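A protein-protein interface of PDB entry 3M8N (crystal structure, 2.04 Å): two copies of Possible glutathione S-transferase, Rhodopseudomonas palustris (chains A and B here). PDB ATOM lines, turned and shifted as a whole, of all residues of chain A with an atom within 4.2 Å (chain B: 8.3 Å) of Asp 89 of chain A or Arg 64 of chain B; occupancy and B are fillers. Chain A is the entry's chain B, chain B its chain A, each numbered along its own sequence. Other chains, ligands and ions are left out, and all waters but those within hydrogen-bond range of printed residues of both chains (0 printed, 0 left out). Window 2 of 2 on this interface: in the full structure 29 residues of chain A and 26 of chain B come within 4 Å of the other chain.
Of the 10 printed residues of chain A, 6 touch a printed residue of chain B.
Printed residues of chain A that touch a printed residue of chain B: Arg 87, Met 88, Asp 89, Arg 90, Ala 91 and Glu 92.
Hydrophobic or aromatic side chains of chain A within 4 Å of the printed part of chain B: Met 88 and Ala 91.
Among the printed residues, Asp or Glu carboxylates within 4 Å of a Lys or Arg side-chain nitrogen of the other chain: Asp 89 of chain A with Arg 64 of chain B (3.4 Å) and Glu 92 of chain A with Arg 64 of chain B (3.6 Å).
The side-chain carboxylate of Glu 92 of chain A sits at hydrogen-bond distance from the backbone NH of Ala 155 of chain A.
O of Leu 58 of chain B is in hydrogen-bond range of N of Leu 66 of chain B (2.8 Å).
OG1 of Thr 86 of chain A is in hydrogen-bond range of N of Asp 89 of chain A, at 3.1 Å.
Among the printed residues, pairs that only touch across the chains: Met 88 of chain A with Thr 60 of chain B (3.1 Å), Arg 87 of chain A with Trp 74 of chain B (3.6 Å), Ala 91 of chain A with Leu 66 of chain B (3.6 Å), Ala 91 of chain A with Trp 74 of chain B (3.6 Å), Met 88 of chain A with Tyr 75 of chain B (3.6 Å), Arg 90 of chain A with Trp 74 of chain B (3.7 Å) and Ala 91 of chain A with Tyr 75 of chain B (3.9 Å).
Thr 86 of chain A touches none of the printed residues of chain B.
Of the printed residues of chain B, Arg 87 of chain A touches Trp 74 (3.6 Å) and Tyr 75 (2.9 Å).
Met 88 of chain A touches just these residues of chain B: Thr 60, Arg 64 and Tyr 75.
Of chain B, only Arg 64 (3.4 Å) comes within 4 Å of Asp 89 of chain A.
Tyr 7 of chain B touches none of the printed residues of chain A.
Printed residues of chain A within 4 Å of Thr 60 of chain B: Met 88.
Arg 64 of chain B touches just these residues of chain A: Met 88 (3.0 Å), Asp 89 (3.4 Å) and Glu 92 (3.6 Å).
The nearest residue of chain B that does not touch Asp 89 of chain A is Tyr 75 of chain B (6.3 Å).
The nearest printed residue of chain B that does not touch Glu 92 of chain A is Leu 66 of chain B (4.1 Å).
No position is printed for both chains.
The guanidinium group (NH2) of Arg 64 of chain B lies within salt-bridge range of the side-chain carboxylate (OD1) of Asp 89 of chain A, at 3.4 Å.
The guanidinium group (NH1) of Arg 64 of chain B lies close to the side-chain sulfur (SD) of Met 88 of chain A (3.4 Å).
The side-chain carboxylate (OE1) of Glu 92 of chain A is in salt-bridge range of the guanidinium group (NH2) of Arg 64 of chain B.
O of Tyr 75 of chain B is in hydrogen-bond range of NH2 of Arg 87 of chain A, 2.9 Å away.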
ATOM      1  N   PRO A  84      -6.182   9.058  23.658  1.00  0.00           N
ATOM      2  CA  PRO A  84      -6.641   8.077  22.756  1.00  0.00           C
ATOM      3  C   PRO A  84      -6.934   6.698  23.403  1.00  0.00           C
ATOM      4  O   PRO A  84      -6.649   6.438  24.553  1.00  0.00           O
ATOM      5  CB  PRO A  84      -5.500   8.009  21.720  1.00  0.00           C
ATOM      6  CG  PRO A  84      -4.381   8.503  22.357  1.00  0.00           C
ATOM      7  CD  PRO A  84      -4.772   9.383  23.422  1.00  0.00           C
ATOM      8  N   THR A  86      -6.187   3.173  22.456  1.00  0.00           N
ATOM      9  CA  THR A  86      -5.459   1.977  22.663  1.00  0.00           C
ATOM     10  C   THR A  86      -4.122   2.254  23.323  1.00  0.00           C
ATOM     11  O   THR A  86      -3.667   3.367  23.363  1.00  0.00           O
ATOM     12  CB  THR A  86      -5.223   1.314  21.401  1.00  0.00           C
ATOM     13  OG1 THR A  86      -4.301   2.094  20.657  1.00  0.00           O
ATOM     14  CG2 THR A  86      -6.536   1.128  20.633  1.00  0.00           C
ATOM     15  N   ARG A  87      -3.516   1.203  23.853  1.00  0.00           N
ATOM     16  CA  ARG A  87      -2.208   1.278  24.438  1.00  0.00           C
ATOM     17  C   ARG A  87      -1.173   1.835  23.425  1.00  0.00           C
ATOM     18  O   ARG A  87      -0.363   2.684  23.777  1.00  0.00           O
ATOM     19  CB  ARG A  87      -1.840  -0.123  24.964  1.00  0.00           C
ATOM     20  CG  ARG A  87      -0.592  -0.262  25.729  1.00  0.00           C
ATOM     21  CD  ARG A  87      -0.384  -1.741  25.886  1.00  0.00           C
ATOM     22  NE  ARG A  87       0.882  -2.176  26.430  1.00  0.00           N
ATOM     23  CZ  ARG A  87       1.010  -3.208  27.226  1.00  0.00           C
ATOM     24  NH1 ARG A  87      -0.078  -3.868  27.589  1.00  0.00           N
ATOM     25  NH2 ARG A  87       2.219  -3.521  27.713  1.00  0.00           N
ATOM     26  N   MET A  88      -1.205   1.373  22.179  1.00  0.00           N
ATOM     27  CA  MET A  88      -0.259   1.873  21.201  1.00  0.00           C
ATOM     28  C   MET A  88      -0.460   3.356  20.865  1.00  0.00           C
ATOM     29  O   MET A  88       0.482   4.062  20.731  1.00  0.00           O
ATOM     30  CB  MET A  88      -0.274   1.086  19.918  1.00  0.00           C
ATOM     31  CG  MET A  88       0.748  -0.007  19.812  1.00  0.00           C
ATOM     32  SD  MET A  88       0.450  -1.231  18.178  1.00  0.00           S
ATOM     33  CE  MET A  88      -1.507  -1.077  17.976  1.00  0.00           C
ATOM     34  N   ASP A  89      -1.688   3.803  20.720  1.00  0.00           N
ATOM     35  CA  ASP A  89      -1.990   5.198  20.450  1.00  0.00           C
ATOM     36  C   ASP A  89      -1.611   6.086  21.603  1.00  0.00           C
ATOM     37  O   ASP A  89      -1.093   7.179  21.395  1.00  0.00           O
ATOM     38  CB  ASP A  89      -3.477   5.383  20.230  1.00  0.00           C
ATOM     39  CG  ASP A  89      -3.969   4.875  18.887  1.00  0.00           C
ATOM     40  OD1 ASP A  89      -3.232   4.609  17.940  1.00  0.00           O
ATOM     41  OD2 ASP A  89      -5.175   4.790  18.758  1.00  0.00           O
ATOM     42  N   ARG A  90      -1.871   5.630  22.819  1.00  0.00           N
ATOM     43  CA  ARG A  90      -1.383   6.352  23.990  1.00  0.00           C
ATOM     44  C   ARG A  90       0.131   6.508  24.077  1.00  0.00           C
ATOM     45  O   ARG A  90       0.615   7.569  24.312  1.00  0.00           O
ATOM     46  CB  ARG A  90      -1.972   5.776  25.262  1.00  0.00           C
ATOM     47  CG  ARG A  90      -3.297   6.399  25.480  1.00  0.00           C
ATOM     48  CD  ARG A  90      -4.368   5.467  25.922  1.00  0.00           C
ATOM     49  NE  ARG A  90      -3.982   4.908  27.155  1.00  0.00           N
ATOM     50  CZ  ARG A  90      -4.408   3.764  27.641  1.00  0.00           C
ATOM     51  NH1 ARG A  90      -3.905   3.393  28.816  1.00  0.00           N
ATOM     52  NH2 ARG A  90      -5.288   2.996  26.994  1.00  0.00           N
ATOM     53  N   ALA A  91       0.858   5.438  23.844  1.00  0.00           N
ATOM     54  CA  ALA A  91       2.284   5.500  23.751  1.00  0.00           C
ATOM     55  C   ALA A  91       2.765   6.473  22.673  1.00  0.00           C
ATOM     56  O   ALA A  91       3.759   7.122  22.830  1.00  0.00           O
ATOM     57  CB  ALA A  91       2.867   4.121  23.522  1.00  0.00           C
ATOM     58  N   GLU A  92       2.047   6.529  21.557  1.00  0.00           N
ATOM     59  CA  GLU A  92       2.365   7.384  20.420  1.00  0.00           C
ATOM     60  C   GLU A  92       2.213   8.838  20.840  1.00  0.00           C
ATOM     61  O   GLU A  92       3.010   9.629  20.496  1.00  0.00           O
ATOM     62  CB  GLU A  92       1.500   7.020  19.189  1.00  0.00           C
ATOM     63  CG  GLU A  92       2.039   7.594  17.993  1.00  0.00           C
ATOM     64  CD  GLU A  92       1.141   7.600  16.727  1.00  0.00           C
ATOM     65  OE1 GLU A  92      -0.055   7.206  16.712  1.00  0.00           O
ATOM     66  OE2 GLU A  92       1.700   8.077  15.703  1.00  0.00           O
ATOM     67  N   ALA A  93       1.239   9.153  21.657  1.00  0.00           N
ATOM     68  CA  ALA A  93       1.121  10.455  22.213  1.00  0.00           C
ATOM     69  C   ALA A  93       2.261  10.786  23.172  1.00  0.00           C
ATOM     70  O   ALA A  93       2.872  11.840  23.053  1.00  0.00           O
ATOM     71  CB  ALA A  93      -0.234  10.614  22.924  1.00  0.00           C
ATOM     72  N   ALA A 155      -2.384   9.168  16.954  1.00  0.00           N
ATOM     73  CA  ALA A 155      -3.664   8.444  16.945  1.00  0.00           C
ATOM     74  C   ALA A 155      -4.691   8.917  15.945  1.00  0.00           C
ATOM     75  O   ALA A 155      -5.813   8.565  16.097  1.00  0.00           O
ATOM     76  CB  ALA A 155      -4.316   8.482  18.349  1.00  0.00           C
ATOM     77  N   LYS B   5      10.886  -6.388  18.454  1.00  0.00           N
ATOM     78  CA  LYS B   5      12.173  -6.093  17.883  1.00  0.00           C
ATOM     79  C   LYS B   5      12.623  -4.748  18.405  1.00  0.00           C
ATOM     80  O   LYS B   5      11.902  -3.780  18.244  1.00  0.00           O
ATOM     81  CB  LYS B   5      12.070  -6.050  16.365  1.00  0.00           C
ATOM     82  CG  LYS B   5      13.395  -6.293  15.695  1.00  0.00           C
ATOM     83  CD  LYS B   5      13.371  -6.056  14.204  1.00  0.00           C
ATOM     84  CE  LYS B   5      12.428  -6.935  13.513  1.00  0.00           C
ATOM     85  NZ  LYS B   5      12.794  -7.020  12.064  1.00  0.00           N
ATOM     86  N   TYR B   7      15.645  -1.922  18.021  1.00  0.00           N
ATOM     87  CA  TYR B   7      16.823  -1.344  17.424  1.00  0.00           C
ATOM     88  C   TYR B   7      17.490  -0.545  18.508  1.00  0.00           C
ATOM     89  O   TYR B   7      16.875   0.325  19.125  1.00  0.00           O
ATOM     90  CB  TYR B   7      16.455  -0.455  16.247  1.00  0.00           C
ATOM     91  CG  TYR B   7      15.783  -1.191  15.089  1.00  0.00           C
ATOM     92  CD1 TYR B   7      16.499  -1.555  13.957  1.00  0.00           C
ATOM     93  CD2 TYR B   7      14.406  -1.492  15.129  1.00  0.00           C
ATOM     94  CE1 TYR B   7      15.875  -2.207  12.910  1.00  0.00           C
ATOM     95  CE2 TYR B   7      13.776  -2.124  14.107  1.00  0.00           C
ATOM     96  CZ  TYR B   7      14.513  -2.495  13.001  1.00  0.00           C
ATOM     97  OH  TYR B   7      13.857  -3.140  11.984  1.00  0.00           O
ATOM     98  N   LYS B  49      11.982   3.693   8.846  1.00  0.00           N
ATOM     99  CA  LYS B  49      11.230   3.261  10.059  1.00  0.00           C
ATOM    100  C   LYS B  49      11.114   4.369  11.105  1.00  0.00           C
ATOM    101  O   LYS B  49      10.089   4.513  11.771  1.00  0.00           O
ATOM    102  CB  LYS B  49      11.920   2.077  10.693  1.00  0.00           C
ATOM    103  CG  LYS B  49      12.405   1.097   9.738  1.00  0.00           C
ATOM    104  CD  LYS B  49      13.623   0.471  10.336  1.00  0.00           C
ATOM    105  CE  LYS B  49      14.348  -0.449   9.354  1.00  0.00           C
ATOM    106  NZ  LYS B  49      13.813  -1.824   9.405  1.00  0.00           N
ATOM    107  N   LEU B  57      14.351   2.130  18.949  1.00  0.00           N
ATOM    108  CA  LEU B  57      13.082   2.056  18.280  1.00  0.00           C
ATOM    109  C   LEU B  57      12.508   0.709  18.562  1.00  0.00           C
ATOM    110  O   LEU B  57      13.190  -0.298  18.434  1.00  0.00           O
ATOM    111  CB  LEU B  57      13.288   2.202  16.789  1.00  0.00           C
ATOM    112  CG  LEU B  57      12.184   2.755  15.895  1.00  0.00           C
ATOM    113  CD1 LEU B  57      11.797   4.150  16.288  1.00  0.00           C
ATOM    114  CD2 LEU B  57      12.738   2.770  14.504  1.00  0.00           C
ATOM    115  N   LEU B  58      11.243   0.694  18.969  1.00  0.00           N
ATOM    116  CA  LEU B  58      10.545  -0.538  19.228  1.00  0.00           C
ATOM    117  C   LEU B  58       9.511  -0.809  18.166  1.00  0.00           C
ATOM    118  O   LEU B  58       8.539  -0.123  18.093  1.00  0.00           O
ATOM    119  CB  LEU B  58       9.820  -0.460  20.569  1.00  0.00           C
ATOM    120  CG  LEU B  58       9.166  -1.704  21.122  1.00  0.00           C
ATOM    121  CD1 LEU B  58      10.251  -2.588  21.492  1.00  0.00           C
ATOM    122  CD2 LEU B  58       8.276  -1.380  22.322  1.00  0.00           C
ATOM    123  N   GLU B  59       9.722  -1.844  17.357  1.00  0.00           N
ATOM    124  CA  GLU B  59       8.660  -2.359  16.463  1.00  0.00           C
ATOM    125  C   GLU B  59       7.608  -3.090  17.217  1.00  0.00           C
ATOM    126  O   GLU B  59       7.870  -4.163  17.788  1.00  0.00           O
ATOM    127  CB  GLU B  59       9.187  -3.444  15.541  1.00  0.00           C
ATOM    128  CG  GLU B  59       9.734  -3.010  14.237  1.00  0.00           C
ATOM    129  CD  GLU B  59       9.576  -4.057  13.133  1.00  0.00           C
ATOM    130  OE1 GLU B  59       8.407  -4.437  12.843  1.00  0.00           O
ATOM    131  OE2 GLU B  59      10.630  -4.445  12.544  1.00  0.00           O
ATOM    132  N   THR B  60       6.419  -2.533  17.212  1.00  0.00           N
ATOM    133  CA  THR B  60       5.234  -3.270  17.604  1.00  0.00           C
ATOM    134  C   THR B  60       4.671  -4.262  16.542  1.00  0.00           C
ATOM    135  O   THR B  60       5.074  -5.447  16.401  1.00  0.00           O
ATOM    136  CB  THR B  60       4.161  -2.296  17.772  1.00  0.00           C
ATOM    137  OG1 THR B  60       4.572  -1.325  18.743  1.00  0.00           O
ATOM    138  CG2 THR B  60       2.900  -3.057  18.185  1.00  0.00           C
ATOM    139  N   ALA B  61       3.695  -3.726  15.821  1.00  0.00           N
ATOM    140  CA  ALA B  61       3.137  -4.298  14.601  1.00  0.00           C
ATOM    141  C   ALA B  61       4.238  -4.390  13.535  1.00  0.00           C
ATOM    142  O   ALA B  61       5.276  -3.779  13.696  1.00  0.00           O
ATOM    143  CB  ALA B  61       1.981  -3.376  14.131  1.00  0.00           C
ATOM    144  N   PRO B  62       4.029  -5.151  12.436  1.00  0.00           N
ATOM    145  CA  PRO B  62       5.064  -5.050  11.372  1.00  0.00           C
ATOM    146  C   PRO B  62       4.984  -3.685  10.700  1.00  0.00           C
ATOM    147  O   PRO B  62       3.894  -3.219  10.401  1.00  0.00           O
ATOM    148  CB  PRO B  62       4.692  -6.174  10.409  1.00  0.00           C
ATOM    149  CG  PRO B  62       3.863  -7.108  11.259  1.00  0.00           C
ATOM    150  CD  PRO B  62       3.061  -6.214  12.136  1.00  0.00           C
ATOM    151  N   GLY B  63       6.129  -3.023  10.548  1.00  0.00           N
ATOM    152  CA  GLY B  63       6.157  -1.624  10.114  1.00  0.00           C
ATOM    153  C   GLY B  63       5.496  -0.562  10.984  1.00  0.00           C
ATOM    154  O   GLY B  63       5.084   0.461  10.483  1.00  0.00           O
ATOM    155  N   ARG B  64       5.399  -0.802  12.281  1.00  0.00           N
ATOM    156  CA  ARG B  64       4.994   0.215  13.201  1.00  0.00           C
ATOM    157  C   ARG B  64       6.009   0.351  14.344  1.00  0.00           C
ATOM    158  O   ARG B  64       6.235  -0.561  15.098  1.00  0.00           O
ATOM    159  CB  ARG B  64       3.598  -0.056  13.727  1.00  0.00           C
ATOM    160  CG  ARG B  64       2.994   1.218  14.332  1.00  0.00           C
ATOM    161  CD  ARG B  64       1.598   1.058  14.893  1.00  0.00           C
ATOM    162  NE  ARG B  64       1.201   2.293  15.556  1.00  0.00           N
ATOM    163  CZ  ARG B  64       0.079   2.440  16.269  1.00  0.00           C
ATOM    164  NH1 ARG B  64      -0.773   1.416  16.388  1.00  0.00           N
ATOM    165  NH2 ARG B  64      -0.212   3.622  16.844  1.00  0.00           N
ATOM    166  N   TYR B  65       6.610   1.521  14.444  1.00  0.00           N
ATOM    167  CA  TYR B  65       7.726   1.804  15.352  1.00  0.00           C
ATOM    168  C   TYR B  65       7.446   2.846  16.424  1.00  0.00           C
ATOM    169  O   TYR B  65       6.962   3.921  16.153  1.00  0.00           O
ATOM    170  CB  TYR B  65       8.886   2.257  14.516  1.00  0.00           C
ATOM    171  CG  TYR B  65       9.190   1.271  13.447  1.00  0.00           C
ATOM    172  CD1 TYR B  65      10.031   0.178  13.699  1.00  0.00           C
ATOM    173  CD2 TYR B  65       8.622   1.382  12.201  1.00  0.00           C
ATOM    174  CE1 TYR B  65      10.299  -0.744  12.726  1.00  0.00           C
ATOM    175  CE2 TYR B  65       8.896   0.452  11.200  1.00  0.00           C
ATOM    176  CZ  TYR B  65       9.721  -0.607  11.479  1.00  0.00           C
ATOM    177  OH  TYR B  65       9.978  -1.530  10.508  1.00  0.00           O
ATOM    178  N   LEU B  66       7.746   2.539  17.652  1.00  0.00           N
ATOM    179  CA  LEU B  66       7.628   3.514  18.663  1.00  0.00           C
ATOM    180  C   LEU B  66       9.013   4.014  19.023  1.00  0.00           C
ATOM    181  O   LEU B  66       9.936   3.256  19.152  1.00  0.00           O
ATOM    182  CB  LEU B  66       6.871   2.911  19.845  1.00  0.00           C
ATOM    183  CG  LEU B  66       6.747   3.687  21.124  1.00  0.00           C
ATOM    184  CD1 LEU B  66       5.754   4.786  20.949  1.00  0.00           C
ATOM    185  CD2 LEU B  66       6.338   2.731  22.126  1.00  0.00           C
ATOM    186  N   ALA B  67       9.166   5.332  19.072  1.00  0.00           N
ATOM    187  CA  ALA B  67      10.420   5.961  19.373  1.00  0.00           C
ATOM    188  C   ALA B  67      10.349   6.590  20.721  1.00  0.00           C
ATOM    189  O   ALA B  67       9.300   6.650  21.322  1.00  0.00           O
ATOM    190  CB  ALA B  67      10.726   6.994  18.371  1.00  0.00           C
ATOM    191  N   TRP B  74       7.063   3.297  29.001  1.00  0.00           N
ATOM    192  CA  TRP B  74       5.668   3.316  29.372  1.00  0.00           C
ATOM    193  C   TRP B  74       4.847   2.204  28.685  1.00  0.00           C
ATOM    194  O   TRP B  74       4.052   1.534  29.337  1.00  0.00           O
ATOM    195  CB  TRP B  74       5.067   4.688  29.094  1.00  0.00           C
ATOM    196  CG  TRP B  74       3.634   4.761  29.518  1.00  0.00           C
ATOM    197  CD1 TRP B  74       3.154   5.204  30.722  1.00  0.00           C
ATOM    198  CD2 TRP B  74       2.487   4.371  28.753  1.00  0.00           C
ATOM    199  NE1 TRP B  74       1.806   5.125  30.750  1.00  0.00           N
ATOM    200  CE2 TRP B  74       1.353   4.624  29.554  1.00  0.00           C
ATOM    201  CE3 TRP B  74       2.299   3.881  27.431  1.00  0.00           C
ATOM    202  CZ2 TRP B  74      -0.004   4.344  29.090  1.00  0.00           C
ATOM    203  CZ3 TRP B  74       0.970   3.602  26.962  1.00  0.00           C
ATOM    204  CH2 TRP B  74      -0.164   3.828  27.814  1.00  0.00           C
ATOM    205  N   TYR B  75       5.057   2.054  27.389  1.00  0.00           N
ATOM    206  CA  TYR B  75       4.394   1.094  26.602  1.00  0.00           C
ATOM    207  C   TYR B  75       4.621  -0.325  27.131  1.00  0.00           C
ATOM    208  O   TYR B  75       3.731  -1.140  27.173  1.00  0.00           O
ATOM    209  CB  TYR B  75       4.840   1.191  25.145  1.00  0.00           C
ATOM    210  CG  TYR B  75       4.118   0.170  24.261  1.00  0.00           C
ATOM    211  CD1 TYR B  75       2.749   0.296  23.950  1.00  0.00           C
ATOM    212  CD2 TYR B  75       4.759  -0.952  23.800  1.00  0.00           C
ATOM    213  CE1 TYR B  75       2.079  -0.636  23.155  1.00  0.00           C
ATOM    214  CE2 TYR B  75       4.063  -1.902  23.038  1.00  0.00           C
ATOM    215  CZ  TYR B  75       2.743  -1.706  22.706  1.00  0.00           C
ATOM    216  OH  TYR B  75       2.071  -2.611  21.968  1.00  0.00           O
